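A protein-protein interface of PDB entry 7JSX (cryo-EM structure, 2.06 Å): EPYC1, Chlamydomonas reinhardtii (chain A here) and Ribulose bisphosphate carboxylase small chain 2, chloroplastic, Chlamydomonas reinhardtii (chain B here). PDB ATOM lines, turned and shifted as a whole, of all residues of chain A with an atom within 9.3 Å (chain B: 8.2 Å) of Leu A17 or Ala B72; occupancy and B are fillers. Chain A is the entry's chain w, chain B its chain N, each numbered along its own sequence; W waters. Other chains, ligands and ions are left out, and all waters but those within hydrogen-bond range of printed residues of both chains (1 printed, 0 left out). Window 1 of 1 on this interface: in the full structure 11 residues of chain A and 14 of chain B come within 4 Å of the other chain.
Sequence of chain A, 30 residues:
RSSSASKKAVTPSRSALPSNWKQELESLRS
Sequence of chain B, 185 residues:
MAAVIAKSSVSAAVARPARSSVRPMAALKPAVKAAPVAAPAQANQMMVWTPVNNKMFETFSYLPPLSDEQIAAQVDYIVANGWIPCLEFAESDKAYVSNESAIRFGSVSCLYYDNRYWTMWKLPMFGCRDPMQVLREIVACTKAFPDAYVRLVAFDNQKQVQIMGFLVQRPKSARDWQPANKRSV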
ATOM      1  N   PRO A  12      -4.760  28.687  33.348  1.00  0.00           N
ATOM      2  CA  PRO A  12      -5.070  28.573  31.920  1.00  0.00           C
ATOM      3  C   PRO A  12      -5.462  29.916  31.291  1.00  0.00           C
ATOM      4  O   PRO A  12      -6.603  30.310  31.446  1.00  0.00           O
ATOM      5  CB  PRO A  12      -6.327  27.693  31.890  1.00  0.00           C
ATOM      6  CG  PRO A  12      -6.352  27.013  33.237  1.00  0.00           C
ATOM      7  CD  PRO A  12      -5.746  28.019  34.191  1.00  0.00           C
ATOM      8  N   SER A  13      -4.526  30.578  30.606  1.00  0.00           N
ATOM      9  CA  SER A  13      -4.877  31.861  29.944  1.00  0.00           C
ATOM     10  C   SER A  13      -5.657  31.532  28.669  1.00  0.00           C
ATOM     11  O   SER A  13      -5.227  30.618  27.940  1.00  0.00           O
ATOM     12  CB  SER A  13      -3.629  32.686  29.623  1.00  0.00           C
ATOM     13  OG  SER A  13      -2.786  32.002  28.712  1.00  0.00           O
ATOM     14  N   ARG A  14      -6.769  32.217  28.417  1.00  0.00           N
ATOM     15  CA  ARG A  14      -7.591  31.950  27.235  1.00  0.00           C
ATOM     16  C   ARG A  14      -6.985  32.391  25.894  1.00  0.00           C
ATOM     17  O   ARG A  14      -6.185  33.323  25.817  1.00  0.00           O
ATOM     18  CB  ARG A  14      -9.008  32.505  27.410  1.00  0.00           C
ATOM     19  CG  ARG A  14      -9.958  32.137  26.283  1.00  0.00           C
ATOM     20  CD  ARG A  14     -10.172  30.633  26.181  1.00  0.00           C
ATOM     21  NE  ARG A  14     -11.187  30.153  27.111  1.00  0.00           N
ATOM     22  CZ  ARG A  14     -10.928  29.635  28.307  1.00  0.00           C
ATOM     23  NH1 ARG A  14      -9.675  29.515  28.724  1.00  0.00           N
ATOM     24  NH2 ARG A  14     -11.921  29.236  29.083  1.00  0.00           N
ATOM     25  N   SER A  15      -7.392  31.683  24.848  1.00  0.00           N
ATOM     26  CA  SER A  15      -6.966  31.879  23.486  1.00  0.00           C
ATOM     27  C   SER A  15      -8.207  32.129  22.637  1.00  0.00           C
ATOM     28  O   SER A  15      -9.044  31.246  22.480  1.00  0.00           O
ATOM     29  CB  SER A  15      -6.258  30.619  22.967  1.00  0.00           C
ATOM     30  OG  SER A  15      -5.089  30.320  23.712  1.00  0.00           O
ATOM     31  N   ALA A  16      -8.372  33.378  22.233  1.00  0.00           N
ATOM     32  CA  ALA A  16      -9.503  33.695  21.410  1.00  0.00           C
ATOM     33  C   ALA A  16      -9.210  32.903  20.163  1.00  0.00           C
ATOM     34  O   ALA A  16      -8.091  32.916  19.649  1.00  0.00           O
ATOM     35  CB  ALA A  16      -9.642  35.187  21.145  1.00  0.00           C
ATOM     36  N   LEU A  17     -10.219  32.198  19.681  1.00  0.00           N
ATOM     37  CA  LEU A  17     -10.080  31.418  18.474  1.00  0.00           C
ATOM     38  C   LEU A  17     -10.180  32.354  17.280  1.00  0.00           C
ATOM     39  O   LEU A  17     -10.712  33.462  17.385  1.00  0.00           O
ATOM     40  CB  LEU A  17     -11.142  30.319  18.418  1.00  0.00           C
ATOM     41  CG  LEU A  17     -10.817  29.055  19.220  1.00  0.00           C
ATOM     42  CD1 LEU A  17      -9.942  29.361  20.423  1.00  0.00           C
ATOM     43  CD2 LEU A  17     -12.078  28.315  19.639  1.00  0.00           C
ATOM     44  N   PRO A  18      -9.720  31.899  16.110  1.00  0.00           N
ATOM     45  CA  PRO A  18      -9.795  32.740  14.915  1.00  0.00           C
ATOM     46  C   PRO A  18     -11.254  33.049  14.586  1.00  0.00           C
ATOM     47  O   PRO A  18     -12.121  32.198  14.742  1.00  0.00           O
ATOM     48  CB  PRO A  18      -9.182  31.855  13.826  1.00  0.00           C
ATOM     49  CG  PRO A  18      -8.301  30.905  14.562  1.00  0.00           C
ATOM     50  CD  PRO A  18      -8.999  30.639  15.862  1.00  0.00           C
ATOM     51  N   SER A  19     -11.521  34.206  13.991  1.00  0.00           N
ATOM     52  CA  SER A  19     -12.900  34.631  13.731  1.00  0.00           C
ATOM     53  C   SER A  19     -13.734  33.641  12.906  1.00  0.00           C
ATOM     54  O   SER A  19     -14.926  33.473  13.158  1.00  0.00           O
ATOM     55  CB  SER A  19     -12.896  35.989  13.026  1.00  0.00           C
ATOM     56  OG  SER A  19     -12.316  35.892  11.736  1.00  0.00           O
ATOM     57  N   ASN A  20     -13.109  32.978  11.943  1.00  0.00           N
ATOM     58  CA  ASN A  20     -13.788  32.003  11.111  1.00  0.00           C
ATOM     59  C   ASN A  20     -13.744  30.582  11.685  1.00  0.00           C
ATOM     60  O   ASN A  20     -14.072  29.637  10.982  1.00  0.00           O
ATOM     61  CB  ASN A  20     -13.216  32.019   9.691  1.00  0.00           C
ATOM     62  CG  ASN A  20     -13.622  33.254   8.911  1.00  0.00           C
ATOM     63  OD1 ASN A  20     -14.314  34.131   9.430  1.00  0.00           O
ATOM     64  ND2 ASN A  20     -13.195  33.328   7.656  1.00  0.00           N
ATOM     65  N   TRP A  21     -13.359  30.414  12.952  1.00  0.00           N
ATOM     66  CA  TRP A  21     -13.268  29.062  13.514  1.00  0.00           C
ATOM     67  C   TRP A  21     -14.601  28.308  13.452  1.00  0.00           C
ATOM     68  O   TRP A  21     -14.608  27.109  13.186  1.00  0.00           O
ATOM     69  CB  TRP A  21     -12.633  29.032  14.928  1.00  0.00           C
ATOM     70  CG  TRP A  21     -13.572  29.232  16.108  1.00  0.00           C
ATOM     71  CD1 TRP A  21     -14.057  30.416  16.583  1.00  0.00           C
ATOM     72  CD2 TRP A  21     -14.139  28.212  16.940  1.00  0.00           C
ATOM     73  NE1 TRP A  21     -14.880  30.200  17.657  1.00  0.00           N
ATOM     74  CE2 TRP A  21     -14.949  28.853  17.898  1.00  0.00           C
ATOM     75  CE3 TRP A  21     -14.037  26.818  16.970  1.00  0.00           C
ATOM     76  CZ2 TRP A  21     -15.650  28.151  18.873  1.00  0.00           C
ATOM     77  CZ3 TRP A  21     -14.735  26.124  17.939  1.00  0.00           C
ATOM     78  CH2 TRP A  21     -15.532  26.793  18.878  1.00  0.00           C
ATOM     79  N   LYS A  22     -15.720  28.978  13.705  1.00  0.00           N
ATOM     80  CA  LYS A  22     -16.999  28.301  13.606  1.00  0.00           C
ATOM     81  C   LYS A  22     -17.225  27.888  12.156  1.00  0.00           C
ATOM     82  O   LYS A  22     -17.653  26.771  11.872  1.00  0.00           O
ATOM     83  CB  LYS A  22     -18.125  29.223  14.064  1.00  0.00           C
ATOM     84  CG  LYS A  22     -18.124  29.521  15.552  1.00  0.00           C
ATOM     85  CD  LYS A  22     -18.444  28.272  16.351  1.00  0.00           C
ATOM     86  CE  LYS A  22     -18.835  28.612  17.779  1.00  0.00           C
ATOM     87  NZ  LYS A  22     -19.180  27.386  18.546  1.00  0.00           N
ATOM     88  N   GLU A  24     -14.889  27.538   9.765  1.00  0.00           N
ATOM     89  CA  GLU A  24     -13.860  26.597   9.338  1.00  0.00           C
ATOM     90  C   GLU A  24     -14.280  25.190   9.698  1.00  0.00           C
ATOM     91  O   GLU A  24     -14.139  24.262   8.902  1.00  0.00           O
ATOM     92  CB  GLU A  24     -12.536  26.931  10.023  1.00  0.00           C
ATOM     93  CG  GLU A  24     -11.381  26.036   9.614  1.00  0.00           C
ATOM     94  CD  GLU A  24     -10.107  26.368  10.358  1.00  0.00           C
ATOM     95  OE1 GLU A  24     -10.083  27.396  11.065  1.00  0.00           O
ATOM     96  OE2 GLU A  24      -9.129  25.602  10.239  1.00  0.00           O
ATOM     97  N   LEU A  25     -14.804  25.041  10.907  1.00  0.00           N
ATOM     98  CA  LEU A  25     -15.306  23.771  11.373  1.00  0.00           C
ATOM     99  C   LEU A  25     -16.512  23.338  10.545  1.00  0.00           C
ATOM    100  O   LEU A  25     -16.682  22.148  10.292  1.00  0.00           O
ATOM    101  CB  LEU A  25     -15.647  23.816  12.864  1.00  0.00           C
ATOM    102  CG  LEU A  25     -14.463  23.959  13.824  1.00  0.00           C
ATOM    103  CD1 LEU A  25     -14.921  23.919  15.270  1.00  0.00           C
ATOM    104  CD2 LEU A  25     -13.406  22.897  13.570  1.00  0.00           C
ATOM    105  N   LEU B  66     -19.467  18.401  25.348  1.00  0.00           N
ATOM    106  CA  LEU B  66     -18.754  19.655  25.351  1.00  0.00           C
ATOM    107  C   LEU B  66     -18.865  20.278  23.968  1.00  0.00           C
ATOM    108  O   LEU B  66     -18.615  19.623  22.961  1.00  0.00           O
ATOM    109  CB  LEU B  66     -17.309  19.441  25.731  1.00  0.00           C
ATOM    110  CG  LEU B  66     -16.912  18.636  26.976  1.00  0.00           C
ATOM    111  CD1 LEU B  66     -15.405  18.559  27.060  1.00  0.00           C
ATOM    112  CD2 LEU B  66     -17.466  19.131  28.227  1.00  0.00           C
ATOM    113  N   SER B  67     -19.297  21.524  23.923  1.00  0.00           N
ATOM    114  CA  SER B  67     -19.288  22.278  22.683  1.00  0.00           C
ATOM    115  C   SER B  67     -17.860  22.558  22.238  1.00  0.00           C
ATOM    116  O   SER B  67     -16.894  22.307  22.963  1.00  0.00           O
ATOM    117  CB  SER B  67     -20.058  23.590  22.841  1.00  0.00           C
ATOM    118  OG  SER B  67     -19.435  24.437  23.791  1.00  0.00           O
ATOM    119  N   ASP B  68     -17.751  23.118  21.029  1.00  0.00           N
ATOM    120  CA  ASP B  68     -16.448  23.451  20.464  1.00  0.00           C
ATOM    121  C   ASP B  68     -15.714  24.464  21.325  1.00  0.00           C
ATOM    122  O   ASP B  68     -14.504  24.348  21.519  1.00  0.00           O
ATOM    123  CB  ASP B  68     -16.577  23.993  19.037  1.00  0.00           C
ATOM    124  CG  ASP B  68     -17.172  22.993  18.052  1.00  0.00           C
ATOM    125  OD1 ASP B  68     -17.188  21.779  18.310  1.00  0.00           O
ATOM    126  OD2 ASP B  68     -17.578  23.436  16.961  1.00  0.00           O
ATOM    127  N   GLU B  69     -16.439  25.431  21.893  1.00  0.00           N
ATOM    128  CA  GLU B  69     -15.823  26.380  22.814  1.00  0.00           C
ATOM    129  C   GLU B  69     -15.408  25.700  24.113  1.00  0.00           C
ATOM    130  O   GLU B  69     -14.390  26.057  24.703  1.00  0.00           O
ATOM    131  CB  GLU B  69     -16.777  27.535  23.125  1.00  0.00           C
ATOM    132  CG  GLU B  69     -17.167  28.371  21.952  1.00  0.00           C
ATOM    133  CD  GLU B  69     -17.995  29.594  22.334  1.00  0.00           C
ATOM    134  OE1 GLU B  69     -18.236  29.819  23.539  1.00  0.00           O
ATOM    135  OE2 GLU B  69     -18.428  30.322  21.419  1.00  0.00           O
ATOM    136  N   GLN B  70     -16.199  24.735  24.572  1.00  0.00           N
ATOM    137  CA  GLN B  70     -15.817  23.983  25.756  1.00  0.00           C
ATOM    138  C   GLN B  70     -14.615  23.093  25.485  1.00  0.00           C
ATOM    139  O   GLN B  70     -13.734  23.002  26.330  1.00  0.00           O
ATOM    140  CB  GLN B  70     -17.021  23.217  26.300  1.00  0.00           C
ATOM    141  CG  GLN B  70     -17.938  24.105  27.140  1.00  0.00           C
ATOM    142  CD  GLN B  70     -19.278  23.497  27.396  1.00  0.00           C
ATOM    143  OE1 GLN B  70     -19.717  22.635  26.658  1.00  0.00           O
ATOM    144  NE2 GLN B  70     -19.894  23.867  28.480  1.00  0.00           N
ATOM    145  N   ILE B  71     -14.511  22.514  24.289  1.00  0.00           N
ATOM    146  CA  ILE B  71     -13.330  21.725  23.956  1.00  0.00           C
ATOM    147  C   ILE B  71     -12.108  22.620  23.844  1.00  0.00           C
ATOM    148  O   ILE B  71     -11.045  22.288  24.365  1.00  0.00           O
ATOM    149  CB  ILE B  71     -13.549  20.903  22.681  1.00  0.00           C
ATOM    150  CG1 ILE B  71     -14.673  19.891  22.864  1.00  0.00           C
ATOM    151  CG2 ILE B  71     -12.277  20.147  22.288  1.00  0.00           C
ATOM    152  CD1 ILE B  71     -15.167  19.360  21.668  1.00  0.00           C
ATOM    153  N   ALA B  72     -12.274  23.793  23.231  1.00  0.00           N
ATOM    154  CA  ALA B  72     -11.184  24.746  23.049  1.00  0.00           C
ATOM    155  C   ALA B  72     -10.637  25.237  24.383  1.00  0.00           C
ATOM    156  O   ALA B  72      -9.428  25.364  24.552  1.00  0.00           O
ATOM    157  CB  ALA B  72     -11.680  25.922  22.204  1.00  0.00           C
ATOM    158  N   ALA B  73     -11.511  25.451  25.353  1.00  0.00           N
ATOM    159  CA  ALA B  73     -11.071  25.878  26.671  1.00  0.00           C
ATOM    160  C   ALA B  73     -10.324  24.763  27.420  1.00  0.00           C
ATOM    161  O   ALA B  73      -9.362  25.048  28.130  1.00  0.00           O
ATOM    162  CB  ALA B  73     -12.267  26.368  27.467  1.00  0.00           C
ATOM    163  N   GLN B  74     -10.751  23.499  27.268  1.00  0.00           N
ATOM    164  CA  GLN B  74      -9.980  22.387  27.820  1.00  0.00           C
ATOM    165  C   GLN B  74      -8.616  22.268  27.148  1.00  0.00           C
ATOM    166  O   GLN B  74      -7.634  21.984  27.821  1.00  0.00           O
ATOM    167  CB  GLN B  74     -10.741  21.063  27.683  1.00  0.00           C
ATOM    168  CG  GLN B  74     -12.090  20.981  28.342  1.00  0.00           C
ATOM    169  CD  GLN B  74     -12.046  21.245  29.796  1.00  0.00           C
ATOM    170  OE1 GLN B  74     -12.681  22.145  30.287  1.00  0.00           O
ATOM    171  NE2 GLN B  74     -11.223  20.516  30.483  1.00  0.00           N
ATOM    172  N   VAL B  75      -8.538  22.492  25.831  1.00  0.00           N
ATOM    173  CA  VAL B  75      -7.256  22.449  25.123  1.00  0.00           C
ATOM    174  C   VAL B  75      -6.325  23.569  25.595  1.00  0.00           C
ATOM    175  O   VAL B  75      -5.117  23.365  25.754  1.00  0.00           O
ATOM    176  CB  VAL B  75      -7.478  22.492  23.598  1.00  0.00           C
ATOM    177  CG1 VAL B  75      -6.199  22.582  22.889  1.00  0.00           C
ATOM    178  CG2 VAL B  75      -8.234  21.318  23.118  1.00  0.00           C
ATOM    179  N   ASP B  76      -6.884  24.744  25.881  1.00  0.00           N
ATOM    180  CA  ASP B  76      -6.118  25.805  26.527  1.00  0.00           C
ATOM    181  C   ASP B  76      -5.553  25.390  27.871  1.00  0.00           C
ATOM    182  O   ASP B  76      -4.434  25.763  28.202  1.00  0.00           O
ATOM    183  CB  ASP B  76      -6.984  27.036  26.671  1.00  0.00           C
ATOM    184  CG  ASP B  76      -7.112  27.764  25.370  1.00  0.00           C
ATOM    185  OD1 ASP B  76      -6.136  27.743  24.634  1.00  0.00           O
ATOM    186  OD2 ASP B  76      -8.185  28.276  25.055  1.00  0.00           O
ATOM    187  N   TYR B  77      -6.306  24.620  28.656  1.00  0.00           N
ATOM    188  CA  TYR B  77      -5.773  24.093  29.898  1.00  0.00           C
ATOM    189  C   TYR B  77      -4.626  23.123  29.630  1.00  0.00           C
ATOM    190  O   TYR B  77      -3.595  23.201  30.286  1.00  0.00           O
ATOM    191  CB  TYR B  77      -6.897  23.434  30.702  1.00  0.00           C
ATOM    192  CG  TYR B  77      -6.481  22.880  32.015  1.00  0.00           C
ATOM    193  CD1 TYR B  77      -6.156  23.737  33.050  1.00  0.00           C
ATOM    194  CD2 TYR B  77      -6.446  21.510  32.245  1.00  0.00           C
ATOM    195  CE1 TYR B  77      -5.778  23.278  34.225  1.00  0.00           C
ATOM    196  CE2 TYR B  77      -6.079  21.019  33.467  1.00  0.00           C
ATOM    197  CZ  TYR B  77      -5.736  21.918  34.456  1.00  0.00           C
ATOM    198  OH  TYR B  77      -5.350  21.516  35.693  1.00  0.00           O
ATOM    199  N   ILE B  78      -4.766  22.263  28.611  1.00  0.00           N
ATOM    200  CA  ILE B  78      -3.708  21.329  28.213  1.00  0.00           C
ATOM    201  C   ILE B  78      -2.439  22.068  27.789  1.00  0.00           C
ATOM    202  O   ILE B  78      -1.341  21.745  28.247  1.00  0.00           O
ATOM    203  CB  ILE B  78      -4.214  20.388  27.094  1.00  0.00           C
ATOM    204  CG1 ILE B  78      -5.215  19.371  27.649  1.00  0.00           C
ATOM    205  CG2 ILE B  78      -3.096  19.688  26.414  1.00  0.00           C
ATOM    206  CD1 ILE B  78      -6.106  18.789  26.701  1.00  0.00           C
ATOM    207  N   VAL B  79      -2.584  23.092  26.963  1.00  0.00           N
ATOM    208  CA  VAL B  79      -1.430  23.787  26.390  1.00  0.00           C
ATOM    209  C   VAL B  79      -0.675  24.580  27.452  1.00  0.00           C
ATOM    210  O   VAL B  79       0.552  24.488  27.536  1.00  0.00           O
ATOM    211  CB  VAL B  79      -1.880  24.671  25.213  1.00  0.00           C
ATOM    212  CG1 VAL B  79      -0.786  25.622  24.800  1.00  0.00           C
ATOM    213  CG2 VAL B  79      -2.243  23.812  24.033  1.00  0.00           C
ATOM    214  N   ASP B 130      -1.677  25.995  19.711  1.00  0.00           N
ATOM    215  CA  ASP B 130      -2.925  26.590  19.337  1.00  0.00           C
ATOM    216  C   ASP B 130      -4.048  25.571  19.389  1.00  0.00           C
ATOM    217  O   ASP B 130      -3.896  24.471  18.854  1.00  0.00           O
ATOM    218  CB  ASP B 130      -2.844  27.183  17.933  1.00  0.00           C
ATOM    219  CG  ASP B 130      -4.079  27.928  17.587  1.00  0.00           C
ATOM    220  OD1 ASP B 130      -4.217  29.073  18.040  1.00  0.00           O
ATOM    221  OD2 ASP B 130      -4.953  27.347  16.912  1.00  0.00           O
ATOM    222  N   PRO B 131      -5.200  25.914  19.965  1.00  0.00           N
ATOM    223  CA  PRO B 131      -6.272  24.928  20.094  1.00  0.00           C
ATOM    224  C   PRO B 131      -7.010  24.587  18.816  1.00  0.00           C
ATOM    225  O   PRO B 131      -7.811  23.645  18.821  1.00  0.00           O
ATOM    226  CB  PRO B 131      -7.208  25.568  21.123  1.00  0.00           C
ATOM    227  CG  PRO B 131      -6.893  26.928  21.142  1.00  0.00           C
ATOM    228  CD  PRO B 131      -5.466  27.098  20.797  1.00  0.00           C
ATOM    229  N   MET B 132      -6.763  25.305  17.724  1.00  0.00           N
ATOM    230  CA  MET B 132      -7.556  25.101  16.525  1.00  0.00           C
ATOM    231  C   MET B 132      -7.082  23.867  15.763  1.00  0.00           C
ATOM    232  O   MET B 132      -7.839  23.272  14.998  1.00  0.00           O
ATOM    233  CB  MET B 132      -7.493  26.377  15.670  1.00  0.00           C
ATOM    234  CG  MET B 132      -8.503  26.489  14.590  1.00  0.00           C
ATOM    235  SD  MET B 132     -10.197  26.572  15.143  1.00  0.00           S
ATOM    236  CE  MET B 132     -10.979  25.953  13.653  1.00  0.00           C
ATOM    237  N   GLN B 133      -5.853  23.441  16.014  1.00  0.00           N
ATOM    238  CA  GLN B 133      -5.352  22.196  15.445  1.00  0.00           C
ATOM    239  C   GLN B 133      -6.074  20.975  16.016  1.00  0.00           C
ATOM    240  O   GLN B 133      -6.420  20.060  15.269  1.00  0.00           O
ATOM    241  CB  GLN B 133      -3.871  22.088  15.707  1.00  0.00           C
ATOM    242  CG  GLN B 133      -3.124  23.237  15.190  1.00  0.00           C
ATOM    243  CD  GLN B 133      -1.676  23.145  15.502  1.00  0.00           C
ATOM    244  OE1 GLN B 133      -1.227  22.214  16.177  1.00  0.00           O
ATOM    245  NE2 GLN B 133      -0.911  24.093  14.991  1.00  0.00           N
ATOM    246  N   VAL B 134      -6.326  20.965  17.326  1.00  0.00           N
ATOM    247  CA  VAL B 134      -7.047  19.859  17.940  1.00  0.00           C
ATOM    248  C   VAL B 134      -8.469  19.825  17.426  1.00  0.00           C
ATOM    249  O   VAL B 134      -8.975  18.768  17.047  1.00  0.00           O
ATOM    250  CB  VAL B 134      -6.994  19.959  19.477  1.00  0.00           C
ATOM    251  CG1 VAL B 134      -7.838  18.842  20.121  1.00  0.00           C
ATOM    252  CG2 VAL B 134      -5.609  19.867  19.940  1.00  0.00           C
ATOM    253  N   LEU B 135      -9.090  21.003  17.302  1.00  0.00           N
ATOM    254  CA  LEU B 135     -10.462  21.083  16.811  1.00  0.00           C
ATOM    255  C   LEU B 135     -10.576  20.634  15.361  1.00  0.00           C
ATOM    256  O   LEU B 135     -11.559  19.995  14.992  1.00  0.00           O
ATOM    257  CB  LEU B 135     -11.019  22.496  17.010  1.00  0.00           C
ATOM    258  CG  LEU B 135     -11.744  22.754  18.343  1.00  0.00           C
ATOM    259  CD1 LEU B 135     -10.848  22.776  19.538  1.00  0.00           C
ATOM    260  CD2 LEU B 135     -12.539  24.045  18.286  1.00  0.00           C
ATOM    261  N   ILE B 138     -10.160  16.821  15.506  1.00  0.00           N
ATOM    262  CA  ILE B 138     -11.401  16.205  15.972  1.00  0.00           C
ATOM    263  C   ILE B 138     -12.375  16.034  14.824  1.00  0.00           C
ATOM    264  O   ILE B 138     -12.920  14.946  14.620  1.00  0.00           O
ATOM    265  CB  ILE B 138     -12.024  17.006  17.143  1.00  0.00           C
ATOM    266  CG1 ILE B 138     -11.205  16.848  18.408  1.00  0.00           C
ATOM    267  CG2 ILE B 138     -13.433  16.581  17.431  1.00  0.00           C
ATOM    268  CD1 ILE B 138     -11.599  17.819  19.488  1.00  0.00           C
ATOM    269  N   LEU B 152     -10.307  12.753  23.751  1.00  0.00           N
ATOM    270  CA  LEU B 152      -9.144  13.616  23.779  1.00  0.00           C
ATOM    271  C   LEU B 152      -8.333  13.314  25.020  1.00  0.00           C
ATOM    272  O   LEU B 152      -8.845  13.386  26.143  1.00  0.00           O
ATOM    273  CB  LEU B 152      -9.531  15.088  23.753  1.00  0.00           C
ATOM    274  CG  LEU B 152      -8.404  16.126  23.919  1.00  0.00           C
ATOM    275  CD1 LEU B 152      -7.315  15.918  22.910  1.00  0.00           C
ATOM    276  CD2 LEU B 152      -8.966  17.472  23.717  1.00  0.00           C
ATOM    277  N   PHE B 166     -11.053  12.646  28.229  1.00  0.00           N
ATOM    278  CA  PHE B 166     -12.462  12.952  28.248  1.00  0.00           C
ATOM    279  C   PHE B 166     -12.945  12.849  26.830  1.00  0.00           C
ATOM    280  O   PHE B 166     -12.191  13.065  25.899  1.00  0.00           O
ATOM    281  CB  PHE B 166     -12.800  14.346  28.798  1.00  0.00           C
ATOM    282  CG  PHE B 166     -12.170  15.484  28.051  1.00  0.00           C
ATOM    283  CD1 PHE B 166     -10.920  15.902  28.381  1.00  0.00           C
ATOM    284  CD2 PHE B 166     -12.832  16.125  27.033  1.00  0.00           C
ATOM    285  CE1 PHE B 166     -10.315  16.977  27.691  1.00  0.00           C
ATOM    286  CE2 PHE B 166     -12.222  17.166  26.332  1.00  0.00           C
ATOM    287  CZ  PHE B 166     -10.988  17.599  26.673  1.00  0.00           C
ATOM    288  N   VAL B 168     -14.974  13.618  23.408  1.00  0.00           N
ATOM    289  CA  VAL B 168     -15.372  14.757  22.596  1.00  0.00           C
ATOM    290  C   VAL B 168     -16.412  14.409  21.563  1.00  0.00           C
ATOM    291  O   VAL B 168     -16.965  15.323  20.948  1.00  0.00           O
ATOM    292  CB  VAL B 168     -14.175  15.457  21.908  1.00  0.00           C
ATOM    293  CG1 VAL B 168     -13.212  16.007  22.898  1.00  0.00           C
ATOM    294  CG2 VAL B 168     -13.466  14.562  20.933  1.00  0.00           C
HETATM  295  O   HOH W   1      -8.622  26.915  29.838  1.00  0.00           O
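The side-chain carboxylate of Asp B76 sits at hydrogen-bond distance from the side-chain hydroxyl of Ser A15 (2.9 Å).
The backbone NH of Met B132 is in hydrogen-bond range of the side-chain carboxylate of Asp B130 (2.8 Å).
Tyr B77 touches Pro A12 (CD1 to CG, 3.3 Å).
Ala B73 touches Arg A14 (CB to NH2, 3.3 Å).
Asp B76 touches Arg A14 (OD2 to CD, 3.3 Å).
Ala B72 touches Leu A17.
CD1 of Leu A17 touches CG of Pro B131 (3.97 Å).
Trp A21 touches Met B132 (CB to SD, 3.5 Å).
Trp A21 touches Leu B135.
OE1 of Glu A24 touches CE of Met B132, at 3.1 Å.
CD1 of Leu A25 touches OD2 of Asp B68, at 3.2 Å.
CD2 of Leu A25 touches O of Leu B135 (3.7 Å).
Leu A17 touches just these residues of chain B: Ala B72 (3.5 Å) and Pro B131 (3.97 Å).
Of chain A, only Leu A17 (3.5 Å) comes within 4 Å of Ala B72.
No residue of chain B comes within 4 Å of Ala A16.
No residue of chain B comes within 4 Å of Pro A18.
Of chain A, only Arg A14 (3.3 Å) comes within 4 Å of Ala B73.
No residue of chain A comes within 4 Å of Val B75.
Printed residues of chain B within 4 Å of Ser A15: Asp B76 (2.9 Å).
Of the printed residues of chain B, Pro A12 touches Tyr B77 (3.3 Å).
The nearest residue of chain B that does not touch Leu A17 is Leu B135 (4.5 Å).
The nearest printed residue of chain B that does not touch Ser A15 is Pro B131 (4.2 Å).
Of the 24 printed residues of chain B, 9 touch a printed residue of chain A.
Hydrophobic or aromatic side chains of chain A that line the printed part of chain B: Pro A12, Leu A17, Trp A21 and Leu A25.
Among the printed residues, no Asp or Glu carboxylate lies within 4 Å of a Lys or Arg side-chain nitrogen of the other chain.
Water W1 lies within hydrogen-bond range of O of Ala B73 (2.6 Å), NH1 of Arg A14 (3.0 Å) and N of Tyr B77 (3.5 Å).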
